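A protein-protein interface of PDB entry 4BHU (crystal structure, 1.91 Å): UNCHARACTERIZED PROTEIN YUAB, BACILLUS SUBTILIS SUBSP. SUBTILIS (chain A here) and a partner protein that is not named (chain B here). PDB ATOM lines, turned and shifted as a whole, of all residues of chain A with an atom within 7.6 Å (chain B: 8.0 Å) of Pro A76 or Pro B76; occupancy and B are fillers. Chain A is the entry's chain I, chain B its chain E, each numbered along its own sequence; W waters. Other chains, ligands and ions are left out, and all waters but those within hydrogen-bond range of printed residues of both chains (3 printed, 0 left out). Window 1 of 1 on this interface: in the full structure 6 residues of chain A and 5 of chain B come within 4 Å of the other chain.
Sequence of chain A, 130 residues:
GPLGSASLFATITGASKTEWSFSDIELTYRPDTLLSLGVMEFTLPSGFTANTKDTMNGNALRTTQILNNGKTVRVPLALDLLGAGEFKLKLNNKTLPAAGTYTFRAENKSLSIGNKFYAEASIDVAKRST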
ATOM      1  N   LEU A  37      16.487  36.957  23.452  1.00  0.00           N
ATOM      2  CA  LEU A  37      16.250  35.570  23.092  1.00  0.00           C
ATOM      3  C   LEU A  37      17.549  34.812  23.224  1.00  0.00           C
ATOM      4  O   LEU A  37      18.603  35.336  22.906  1.00  0.00           O
ATOM      5  CB  LEU A  37      15.776  35.431  21.650  1.00  0.00           C
ATOM      6  CG  LEU A  37      14.392  35.986  21.314  1.00  0.00           C
ATOM      7  CD1 LEU A  37      14.090  35.689  19.842  1.00  0.00           C
ATOM      8  CD2 LEU A  37      13.357  35.389  22.205  1.00  0.00           C
ATOM      9  N   GLY A  38      17.469  33.576  23.684  1.00  0.00           N
ATOM     10  CA  GLY A  38      18.666  32.773  23.828  1.00  0.00           C
ATOM     11  C   GLY A  38      18.550  31.719  24.908  1.00  0.00           C
ATOM     12  O   GLY A  38      17.484  31.137  25.105  1.00  0.00           O
ATOM     13  N   VAL A  39      19.665  31.488  25.604  1.00  0.00           N
ATOM     14  CA  VAL A  39      19.756  30.441  26.612  1.00  0.00           C
ATOM     15  C   VAL A  39      20.460  30.975  27.843  1.00  0.00           C
ATOM     16  O   VAL A  39      21.575  31.482  27.762  1.00  0.00           O
ATOM     17  CB  VAL A  39      20.542  29.219  26.059  1.00  0.00           C
ATOM     18  CG1 VAL A  39      20.505  28.056  27.040  1.00  0.00           C
ATOM     19  CG2 VAL A  39      19.951  28.782  24.730  1.00  0.00           C
ATOM     20  N   MET A  40      19.794  30.882  28.982  1.00  0.00           N
ATOM     21  CA  MET A  40      20.357  31.321  30.251  1.00  0.00           C
ATOM     22  C   MET A  40      21.279  30.192  30.718  1.00  0.00           C
ATOM     23  O   MET A  40      20.842  29.047  30.786  1.00  0.00           O
ATOM     24  CB  MET A  40      19.235  31.525  31.258  1.00  0.00           C
ATOM     25  CG  MET A  40      19.680  31.921  32.658  1.00  0.00           C
ATOM     26  SD  MET A  40      20.329  33.774  32.729  1.00  0.00           S
ATOM     27  CE  MET A  40      22.107  33.442  33.540  1.00  0.00           C
ATOM     28  N   GLU A  41      22.541  30.509  31.012  1.00  0.00           N
ATOM     29  CA  GLU A  41      23.525  29.484  31.380  1.00  0.00           C
ATOM     30  C   GLU A  41      24.388  29.886  32.590  1.00  0.00           C
ATOM     31  O   GLU A  41      24.988  30.973  32.616  1.00  0.00           O
ATOM     32  CB  GLU A  41      24.413  29.146  30.181  1.00  0.00           C
ATOM     33  CG  GLU A  41      25.389  28.022  30.453  1.00  0.00           C
ATOM     34  CD  GLU A  41      26.047  27.511  29.200  1.00  0.00           C
ATOM     35  OE1 GLU A  41      25.341  27.359  28.183  1.00  0.00           O
ATOM     36  OE2 GLU A  41      27.262  27.248  29.230  1.00  0.00           O
ATOM     37  N   THR A  64      17.596  17.536  31.806  1.00  0.00           N
ATOM     38  CA  THR A  64      18.106  18.081  30.544  1.00  0.00           C
ATOM     39  C   THR A  64      18.709  19.467  30.734  1.00  0.00           C
ATOM     40  O   THR A  64      19.382  19.988  29.856  1.00  0.00           O
ATOM     41  CB  THR A  64      16.991  18.207  29.503  1.00  0.00           C
ATOM     42  OG1 THR A  64      15.946  19.026  30.043  1.00  0.00           O
ATOM     43  CG2 THR A  64      16.435  16.840  29.152  1.00  0.00           C
ATOM     44  N   GLN A  65      18.437  20.078  31.876  1.00  0.00           N
ATOM     45  CA  GLN A  65      18.977  21.398  32.178  1.00  0.00           C
ATOM     46  C   GLN A  65      20.337  21.359  32.851  1.00  0.00           C
ATOM     47  O   GLN A  65      20.984  22.397  33.025  1.00  0.00           O
ATOM     48  CB  GLN A  65      18.006  22.169  33.072  1.00  0.00           C
ATOM     49  CG  GLN A  65      16.711  22.531  32.375  1.00  0.00           C
ATOM     50  CD  GLN A  65      15.692  23.205  33.299  1.00  0.00           C
ATOM     51  OE1 GLN A  65      15.740  23.051  34.516  1.00  0.00           O
ATOM     52  NE2 GLN A  65      14.757  23.942  32.708  1.00  0.00           N
ATOM     53  N   VAL A  73      24.318  24.722  34.151  1.00  0.00           N
ATOM     54  CA  VAL A  73      22.865  24.736  34.200  1.00  0.00           C
ATOM     55  C   VAL A  73      22.387  25.641  33.077  1.00  0.00           C
ATOM     56  O   VAL A  73      22.765  26.812  33.013  1.00  0.00           O
ATOM     57  CB  VAL A  73      22.345  25.226  35.565  1.00  0.00           C
ATOM     58  CG1 VAL A  73      20.832  25.264  35.559  1.00  0.00           C
ATOM     59  CG2 VAL A  73      22.854  24.310  36.694  1.00  0.00           C
ATOM     60  N   ARG A  74      21.569  25.069  32.198  1.00  0.00           N
ATOM     61  CA  ARG A  74      21.147  25.698  30.949  1.00  0.00           C
ATOM     62  C   ARG A  74      19.628  25.712  30.834  1.00  0.00           C
ATOM     63  O   ARG A  74      18.977  24.658  30.914  1.00  0.00           O
ATOM     64  CB  ARG A  74      21.683  24.878  29.800  1.00  0.00           C
ATOM     65  CG  ARG A  74      22.382  25.645  28.741  1.00  0.00           C
ATOM     66  CD  ARG A  74      23.061  24.663  27.814  1.00  0.00           C
ATOM     67  NE  ARG A  74      24.499  24.877  27.772  1.00  0.00           N
ATOM     68  CZ  ARG A  74      25.334  24.134  27.062  1.00  0.00           C
ATOM     69  NH1 ARG A  74      24.864  23.127  26.344  1.00  0.00           N
ATOM     70  NH2 ARG A  74      26.635  24.395  27.075  1.00  0.00           N
ATOM     71  N   VAL A  75      19.071  26.907  30.641  1.00  0.00           N
ATOM     72  CA  VAL A  75      17.636  27.071  30.451  1.00  0.00           C
ATOM     73  C   VAL A  75      17.361  27.907  29.213  1.00  0.00           C
ATOM     74  O   VAL A  75      17.523  29.137  29.239  1.00  0.00           O
ATOM     75  CB  VAL A  75      16.990  27.746  31.643  1.00  0.00           C
ATOM     76  CG1 VAL A  75      15.481  27.773  31.453  1.00  0.00           C
ATOM     77  CG2 VAL A  75      17.347  26.998  32.931  1.00  0.00           C
ATOM     78  N   PRO A  76      17.003  27.234  28.116  1.00  0.00           N
ATOM     79  CA  PRO A  76      16.675  27.958  26.897  1.00  0.00           C
ATOM     80  C   PRO A  76      15.441  28.794  27.191  1.00  0.00           C
ATOM     81  O   PRO A  76      14.528  28.343  27.904  1.00  0.00           O
ATOM     82  CB  PRO A  76      16.410  26.832  25.880  1.00  0.00           C
ATOM     83  CG  PRO A  76      17.201  25.660  26.405  1.00  0.00           C
ATOM     84  CD  PRO A  76      17.025  25.770  27.891  1.00  0.00           C
ATOM     85  N   LEU A  77      15.458  30.027  26.690  1.00  0.00           N
ATOM     86  CA  LEU A  77      14.488  31.031  27.086  1.00  0.00           C
ATOM     87  C   LEU A  77      13.218  30.904  26.232  1.00  0.00           C
ATOM     88  O   LEU A  77      13.051  31.590  25.220  1.00  0.00           O
ATOM     89  CB  LEU A  77      15.104  32.444  26.982  1.00  0.00           C
ATOM     90  CG  LEU A  77      15.620  33.236  28.193  1.00  0.00           C
ATOM     91  CD1 LEU A  77      15.654  32.515  29.546  1.00  0.00           C
ATOM     92  CD2 LEU A  77      16.985  33.840  27.877  1.00  0.00           C
ATOM     93  N   ALA A  78      12.334  30.005  26.646  1.00  0.00           N
ATOM     94  CA  ALA A  78      10.963  29.978  26.137  1.00  0.00           C
ATOM     95  C   ALA A  78      10.229  31.293  26.440  1.00  0.00           C
ATOM     96  O   ALA A  78      10.615  32.067  27.321  1.00  0.00           O
ATOM     97  CB  ALA A  78      10.188  28.793  26.748  1.00  0.00           C
ATOM     98  N   LEU A  79       9.125  31.519  25.744  1.00  0.00           N
ATOM     99  CA  LEU A  79       8.440  32.807  25.829  1.00  0.00           C
ATOM    100  C   LEU A  79       8.027  33.126  27.258  1.00  0.00           C
ATOM    101  O   LEU A  79       8.050  34.269  27.680  1.00  0.00           O
ATOM    102  CB  LEU A  79       7.205  32.819  24.920  1.00  0.00           C
ATOM    103  CG  LEU A  79       6.387  34.098  24.930  1.00  0.00           C
ATOM    104  CD1 LEU A  79       7.267  35.251  24.481  1.00  0.00           C
ATOM    105  CD2 LEU A  79       5.188  33.968  24.004  1.00  0.00           C
ATOM    106  N   ASP A  80       7.657  32.107  28.016  1.00  0.00           N
ATOM    107  CA  ASP A  80       7.137  32.346  29.362  1.00  0.00           C
ATOM    108  C   ASP A  80       8.254  32.687  30.356  1.00  0.00           C
ATOM    109  O   ASP A  80       7.983  33.079  31.481  1.00  0.00           O
ATOM    110  CB  ASP A  80       6.341  31.112  29.841  1.00  0.00           C
ATOM    111  CG  ASP A  80       7.096  29.817  29.639  1.00  0.00           C
ATOM    112  OD1 ASP A  80       7.232  29.380  28.464  1.00  0.00           O
ATOM    113  OD2 ASP A  80       7.540  29.227  30.637  1.00  0.00           O
ATOM    114  N   LEU A  81       9.506  32.572  29.923  1.00  0.00           N
ATOM    115  CA  LEU A  81      10.657  32.868  30.801  1.00  0.00           C
ATOM    116  C   LEU A  81      11.325  34.216  30.508  1.00  0.00           C
ATOM    117  O   LEU A  81      11.997  34.777  31.372  1.00  0.00           O
ATOM    118  CB  LEU A  81      11.709  31.736  30.684  1.00  0.00           C
ATOM    119  CG  LEU A  81      11.193  30.349  31.065  1.00  0.00           C
ATOM    120  CD1 LEU A  81      12.263  29.262  30.896  1.00  0.00           C
ATOM    121  CD2 LEU A  81      10.690  30.387  32.511  1.00  0.00           C
ATOM    122  N   LEU A  82      11.122  34.742  29.301  1.00  0.00           N
ATOM    123  CA  LEU A  82      11.900  35.876  28.802  1.00  0.00           C
ATOM    124  C   LEU A  82      11.841  37.112  29.686  1.00  0.00           C
ATOM    125  O   LEU A  82      12.830  37.838  29.819  1.00  0.00           O
ATOM    126  CB  LEU A  82      11.434  36.267  27.392  1.00  0.00           C
ATOM    127  CG  LEU A  82      12.090  35.678  26.151  1.00  0.00           C
ATOM    128  CD1 LEU A  82      11.359  36.209  24.914  1.00  0.00           C
ATOM    129  CD2 LEU A  82      13.585  36.003  26.084  1.00  0.00           C
ATOM    130  N   PHE A  87      17.148  35.584  37.390  1.00  0.00           N
ATOM    131  CA  PHE A  87      17.210  34.138  37.447  1.00  0.00           C
ATOM    132  C   PHE A  87      18.020  33.763  38.674  1.00  0.00           C
ATOM    133  O   PHE A  87      19.213  34.060  38.752  1.00  0.00           O
ATOM    134  CB  PHE A  87      17.812  33.567  36.175  1.00  0.00           C
ATOM    135  CG  PHE A  87      16.787  33.247  35.134  1.00  0.00           C
ATOM    136  CD1 PHE A  87      16.329  34.226  34.270  1.00  0.00           C
ATOM    137  CD2 PHE A  87      16.269  31.967  35.030  1.00  0.00           C
ATOM    138  CE1 PHE A  87      15.376  33.933  33.318  1.00  0.00           C
ATOM    139  CE2 PHE A  87      15.314  31.675  34.075  1.00  0.00           C
ATOM    140  CZ  PHE A  87      14.870  32.667  33.222  1.00  0.00           C
ATOM    141  N   LYS A 109      23.350  33.334  26.648  1.00  0.00           N
ATOM    142  CA  LYS A 109      23.883  33.001  25.330  1.00  0.00           C
ATOM    143  C   LYS A 109      22.871  33.392  24.261  1.00  0.00           C
ATOM    144  O   LYS A 109      21.756  32.869  24.241  1.00  0.00           O
ATOM    145  CB  LYS A 109      24.177  31.500  25.213  1.00  0.00           C
ATOM    146  CG  LYS A 109      25.442  31.012  25.911  1.00  0.00           C
ATOM    147  CD  LYS A 109      25.640  29.495  25.723  1.00  0.00           C
ATOM    148  CE  LYS A 109      26.832  29.158  24.815  1.00  0.00           C
ATOM    149  NZ  LYS A 109      27.220  27.699  24.877  1.00  0.00           N
ATOM    150  N   LEU B  37       3.763  29.590  19.852  1.00  0.00           N
ATOM    151  CA  LEU B  37       4.802  30.416  20.433  1.00  0.00           C
ATOM    152  C   LEU B  37       5.606  29.576  21.410  1.00  0.00           C
ATOM    153  O   LEU B  37       6.359  30.108  22.234  1.00  0.00           O
ATOM    154  CB  LEU B  37       4.168  31.582  21.208  1.00  0.00           C
ATOM    155  CG  LEU B  37       3.315  32.561  20.407  1.00  0.00           C
ATOM    156  CD1 LEU B  37       2.391  33.429  21.338  1.00  0.00           C
ATOM    157  CD2 LEU B  37       4.260  33.416  19.570  1.00  0.00           C
ATOM    158  N   GLY B  38       5.442  28.257  21.320  1.00  0.00           N
ATOM    159  CA  GLY B  38       5.931  27.362  22.349  1.00  0.00           C
ATOM    160  C   GLY B  38       7.143  26.508  22.020  1.00  0.00           C
ATOM    161  O   GLY B  38       7.859  26.743  21.051  1.00  0.00           O
ATOM    162  N   VAL B  39       7.355  25.511  22.856  1.00  0.00           N
ATOM    163  CA  VAL B  39       8.435  24.537  22.664  1.00  0.00           C
ATOM    164  C   VAL B  39       8.029  23.534  21.610  1.00  0.00           C
ATOM    165  O   VAL B  39       6.905  23.044  21.606  1.00  0.00           O
ATOM    166  CB  VAL B  39       8.759  23.816  23.999  1.00  0.00           C
ATOM    167  CG1 VAL B  39       9.789  22.676  23.806  1.00  0.00           C
ATOM    168  CG2 VAL B  39       9.259  24.782  25.010  1.00  0.00           C
ATOM    169  N   MET B  40       8.948  23.203  20.706  1.00  0.00           N
ATOM    170  CA  MET B  40       8.688  22.156  19.729  1.00  0.00           C
ATOM    171  C   MET B  40       9.847  21.179  19.827  1.00  0.00           C
ATOM    172  O   MET B  40      10.984  21.622  19.926  1.00  0.00           O
ATOM    173  CB  MET B  40       8.652  22.751  18.336  1.00  0.00           C
ATOM    174  CG  MET B  40       8.174  21.848  17.263  1.00  0.00           C
ATOM    175  SD  MET B  40       9.643  20.696  16.558  1.00  0.00           S
ATOM    176  CE  MET B  40      10.954  22.098  16.175  1.00  0.00           C
ATOM    177  N   GLU B  41       9.580  19.875  19.829  1.00  0.00           N
ATOM    178  CA  GLU B  41      10.697  18.956  19.826  1.00  0.00           C
ATOM    179  C   GLU B  41      10.480  17.726  18.955  1.00  0.00           C
ATOM    180  O   GLU B  41       9.365  17.199  18.852  1.00  0.00           O
ATOM    181  CB  GLU B  41      11.124  18.615  21.269  1.00  0.00           C
ATOM    182  CG  GLU B  41      10.339  17.622  21.987  1.00  0.00           C
ATOM    183  CD  GLU B  41      10.859  17.417  23.435  1.00  0.00           C
ATOM    184  OE1 GLU B  41      11.377  18.364  24.066  1.00  0.00           O
ATOM    185  OE2 GLU B  41      10.734  16.302  23.921  1.00  0.00           O
ATOM    186  N   THR B  64      22.868  23.486  22.145  1.00  0.00           N
ATOM    187  CA  THR B  64      21.808  23.712  23.125  1.00  0.00           C
ATOM    188  C   THR B  64      20.455  23.129  22.690  1.00  0.00           C
ATOM    189  O   THR B  64      19.556  22.958  23.511  1.00  0.00           O
ATOM    190  CB  THR B  64      21.671  25.191  23.481  1.00  0.00           C
ATOM    191  OG1 THR B  64      21.323  25.953  22.313  1.00  0.00           O
ATOM    192  CG2 THR B  64      22.972  25.686  24.043  1.00  0.00           C
ATOM    193  N   GLN B  65      20.323  22.791  21.413  1.00  0.00           N
ATOM    194  CA  GLN B  65      19.075  22.227  20.899  1.00  0.00           C
ATOM    195  C   GLN B  65      19.051  20.712  20.963  1.00  0.00           C
ATOM    196  O   GLN B  65      18.002  20.094  20.797  1.00  0.00           O
ATOM    197  CB  GLN B  65      18.867  22.636  19.438  1.00  0.00           C
ATOM    198  CG  GLN B  65      18.636  24.103  19.222  1.00  0.00           C
ATOM    199  CD  GLN B  65      18.579  24.437  17.750  1.00  0.00           C
ATOM    200  OE1 GLN B  65      19.578  24.304  17.015  1.00  0.00           O
ATOM    201  NE2 GLN B  65      17.400  24.856  17.294  1.00  0.00           N
ATOM    202  N   LEU B  67      19.487  17.227  22.885  1.00  0.00           N
ATOM    203  CA  LEU B  67      19.355  16.766  24.258  1.00  0.00           C
ATOM    204  C   LEU B  67      19.213  15.268  24.305  1.00  0.00           C
ATOM    205  O   LEU B  67      19.075  14.619  23.279  1.00  0.00           O
ATOM    206  CB  LEU B  67      18.118  17.406  24.914  1.00  0.00           C
ATOM    207  CG  LEU B  67      18.117  18.935  24.958  1.00  0.00           C
ATOM    208  CD1 LEU B  67      16.764  19.483  25.474  1.00  0.00           C
ATOM    209  CD2 LEU B  67      19.264  19.421  25.806  1.00  0.00           C
ATOM    210  N   VAL B  73      15.695  16.842  19.669  1.00  0.00           N
ATOM    211  CA  VAL B  73      16.098  18.101  19.090  1.00  0.00           C
ATOM    212  C   VAL B  73      14.982  19.109  19.414  1.00  0.00           C
ATOM    213  O   VAL B  73      13.844  18.933  18.979  1.00  0.00           O
ATOM    214  CB  VAL B  73      16.258  17.977  17.586  1.00  0.00           C
ATOM    215  CG1 VAL B  73      16.608  19.326  16.984  1.00  0.00           C
ATOM    216  CG2 VAL B  73      17.335  16.936  17.258  1.00  0.00           C
ATOM    217  N   ARG B  74      15.311  20.145  20.175  1.00  0.00           N
ATOM    218  CA  ARG B  74      14.281  21.030  20.714  1.00  0.00           C
ATOM    219  C   ARG B  74      14.468  22.477  20.256  1.00  0.00           C
ATOM    220  O   ARG B  74      15.587  22.986  20.231  1.00  0.00           O
ATOM    221  CB  ARG B  74      14.301  20.937  22.240  1.00  0.00           C
ATOM    222  CG  ARG B  74      13.298  21.856  22.935  1.00  0.00           C
ATOM    223  CD  ARG B  74      13.361  21.678  24.443  1.00  0.00           C
ATOM    224  NE  ARG B  74      12.962  20.348  24.857  1.00  0.00           N
ATOM    225  CZ  ARG B  74      13.260  19.819  26.041  1.00  0.00           C
ATOM    226  NH1 ARG B  74      13.967  20.516  26.922  1.00  0.00           N
ATOM    227  NH2 ARG B  74      12.856  18.596  26.344  1.00  0.00           N
ATOM    228  N   VAL B  75      13.361  23.122  19.878  1.00  0.00           N
ATOM    229  CA  VAL B  75      13.318  24.564  19.634  1.00  0.00           C
ATOM    230  C   VAL B  75      12.467  25.201  20.757  1.00  0.00           C
ATOM    231  O   VAL B  75      11.313  24.846  20.900  1.00  0.00           O
ATOM    232  CB  VAL B  75      12.690  24.811  18.234  1.00  0.00           C
ATOM    233  CG1 VAL B  75      12.542  26.290  17.940  1.00  0.00           C
ATOM    234  CG2 VAL B  75      13.556  24.140  17.130  1.00  0.00           C
ATOM    235  N   PRO B  76      13.046  26.087  21.587  1.00  0.00           N
ATOM    236  CA  PRO B  76      12.324  26.586  22.767  1.00  0.00           C
ATOM    237  C   PRO B  76      11.198  27.555  22.444  1.00  0.00           C
ATOM    238  O   PRO B  76      10.299  27.776  23.255  1.00  0.00           O
ATOM    239  CB  PRO B  76      13.410  27.329  23.570  1.00  0.00           C
ATOM    240  CG  PRO B  76      14.518  27.570  22.609  1.00  0.00           C
ATOM    241  CD  PRO B  76      14.471  26.459  21.607  1.00  0.00           C
ATOM    242  N   LEU B  77      11.288  28.191  21.291  1.00  0.00           N
ATOM    243  CA  LEU B  77      10.258  29.152  20.890  1.00  0.00           C
ATOM    244  C   LEU B  77      10.022  28.968  19.414  1.00  0.00           C
ATOM    245  O   LEU B  77      10.725  29.530  18.566  1.00  0.00           O
ATOM    246  CB  LEU B  77      10.649  30.585  21.238  1.00  0.00           C
ATOM    247  CG  LEU B  77       9.501  31.583  21.510  1.00  0.00           C
ATOM    248  CD1 LEU B  77      10.042  32.933  22.033  1.00  0.00           C
ATOM    249  CD2 LEU B  77       8.683  31.796  20.285  1.00  0.00           C
ATOM    250  N   ALA B  78       9.020  28.156  19.126  1.00  0.00           N
ATOM    251  CA  ALA B  78       8.711  27.679  17.784  1.00  0.00           C
ATOM    252  C   ALA B  78       7.465  28.337  17.226  1.00  0.00           C
ATOM    253  O   ALA B  78       6.353  28.088  17.687  1.00  0.00           O
ATOM    254  CB  ALA B  78       8.523  26.167  17.821  1.00  0.00           C
ATOM    255  N   LEU B  79       7.641  29.188  16.227  1.00  0.00           N
ATOM    256  CA  LEU B  79       6.529  29.951  15.679  1.00  0.00           C
ATOM    257  C   LEU B  79       5.660  29.162  14.698  1.00  0.00           C
ATOM    258  O   LEU B  79       6.139  28.348  13.919  1.00  0.00           O
ATOM    259  CB  LEU B  79       7.048  31.200  14.955  1.00  0.00           C
ATOM    260  CG  LEU B  79       7.837  32.209  15.772  1.00  0.00           C
ATOM    261  CD1 LEU B  79       8.200  33.386  14.867  1.00  0.00           C
ATOM    262  CD2 LEU B  79       7.066  32.687  17.015  1.00  0.00           C
ATOM    263  N   SER B 110       3.998  23.230  24.132  1.00  0.00           N
ATOM    264  CA  SER B 110       3.435  24.372  24.879  1.00  0.00           C
ATOM    265  C   SER B 110       2.936  25.445  23.935  1.00  0.00           C
ATOM    266  O   SER B 110       3.253  25.423  22.735  1.00  0.00           O
ATOM    267  CB  SER B 110       4.472  24.964  25.836  1.00  0.00           C
ATOM    268  OG  SER B 110       5.571  25.526  25.135  1.00  0.00           O
ATOM    269  N   LEU B 111       2.139  26.351  24.500  1.00  0.00           N
ATOM    270  CA  LEU B 111       1.708  27.594  23.855  1.00  0.00           C
ATOM    271  C   LEU B 111       1.348  27.409  22.384  1.00  0.00           C
ATOM    272  O   LEU B 111       1.926  28.039  21.512  1.00  0.00           O
ATOM    273  CB  LEU B 111       2.777  28.673  24.020  1.00  0.00           C
ATOM    274  CG  LEU B 111       3.182  29.067  25.452  1.00  0.00           C
ATOM    275  CD1 LEU B 111       4.212  30.202  25.473  1.00  0.00           C
ATOM    276  CD2 LEU B 111       1.954  29.485  26.226  1.00  0.00           C
HETATM  277  O   HOH W   1      16.424  22.051  28.733  1.00  0.00           O
HETATM  278  O   HOH W   2       6.822  27.657  26.194  1.00  0.00           O
HETATM  279  O   HOH W   3       8.115  29.280  24.129  1.00  0.00           O
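Water W2 lies within hydrogen-bond range of the side-chain hydroxyl (OG) of Ser B110 (2.7 Å) and the side-chain carboxylate (OD1) of Asp A80 (2.9 Å).
Water W3 lies within hydrogen-bond range of O of Leu B37, O of Pro B76 and N of Leu A79.
Water W1 bridges the side-chain hydroxyl of Thr A64 and the guanidinium group of Arg B74.
The backbone NH (N) of Leu B37 sits at hydrogen-bond distance from the backbone carbonyl oxygen (O) of Leu B111 (2.9 Å).
The side-chain carboxylate (OE1) of Glu B41 lies within salt-bridge range of the guanidinium group (NE) of Arg B74, 2.7 Å away.
The backbone carbonyl oxygen of Gln B65 sits at hydrogen-bond distance from the backbone NH of Arg B74 (2.8 Å).
O of Val A39 sits at hydrogen-bond distance from N of Lys A109 (2.8 Å).
The guanidinium group of Arg A74 lies within salt-bridge range of the side-chain carboxylate of Glu A41 (2.7 Å).
O of Gln A65 lies within hydrogen-bond range of N of Arg A74.
Of chain B, only Pro B76 (3.8 Å) comes within 4 Å of Pro A76.
Of chain A, only Pro A76 (3.8 Å) and Ala A78 (3.6 Å) come within 4 Å of Pro B76.
Of the printed residues of chain A, Thr B64 touches Val A39 (3.97 Å) and Arg A74 (3.9 Å).
Of the printed residues of chain B, Ala A78 touches Pro B76 (3.6 Å).
Of the printed residues of chain B, Val A39 touches Thr B64.
Of the printed residues of chain A, Arg B74 touches Thr A64.
Met B40 touches none of the printed residues of chain A.
The nearest residue of chain A that does not touch Pro B76 is Leu A77 (4.5 Å).
Among the printed residues, pairs that only touch across the chains: Ala A78 with Pro B76 (3.6 Å), Leu A79 with Leu B37 (3.8 Å), Pro A76 with Pro B76 (3.8 Å), Arg A74 with Thr B64 (3.9 Å), Val A39 with Thr B64 (3.97 Å) and Thr A64 with Arg B74 (3.98 Å).
Hydrophobic or aromatic side chains of chain B that line the printed part of chain A: Leu B37 and Pro B76.
Of the 19 printed residues of chain A, 6 touch a printed residue of chain B.
Among the printed residues, no Asp or Glu carboxylate lies within 4 Å of a Lys or Arg side-chain nitrogen of the other chain.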
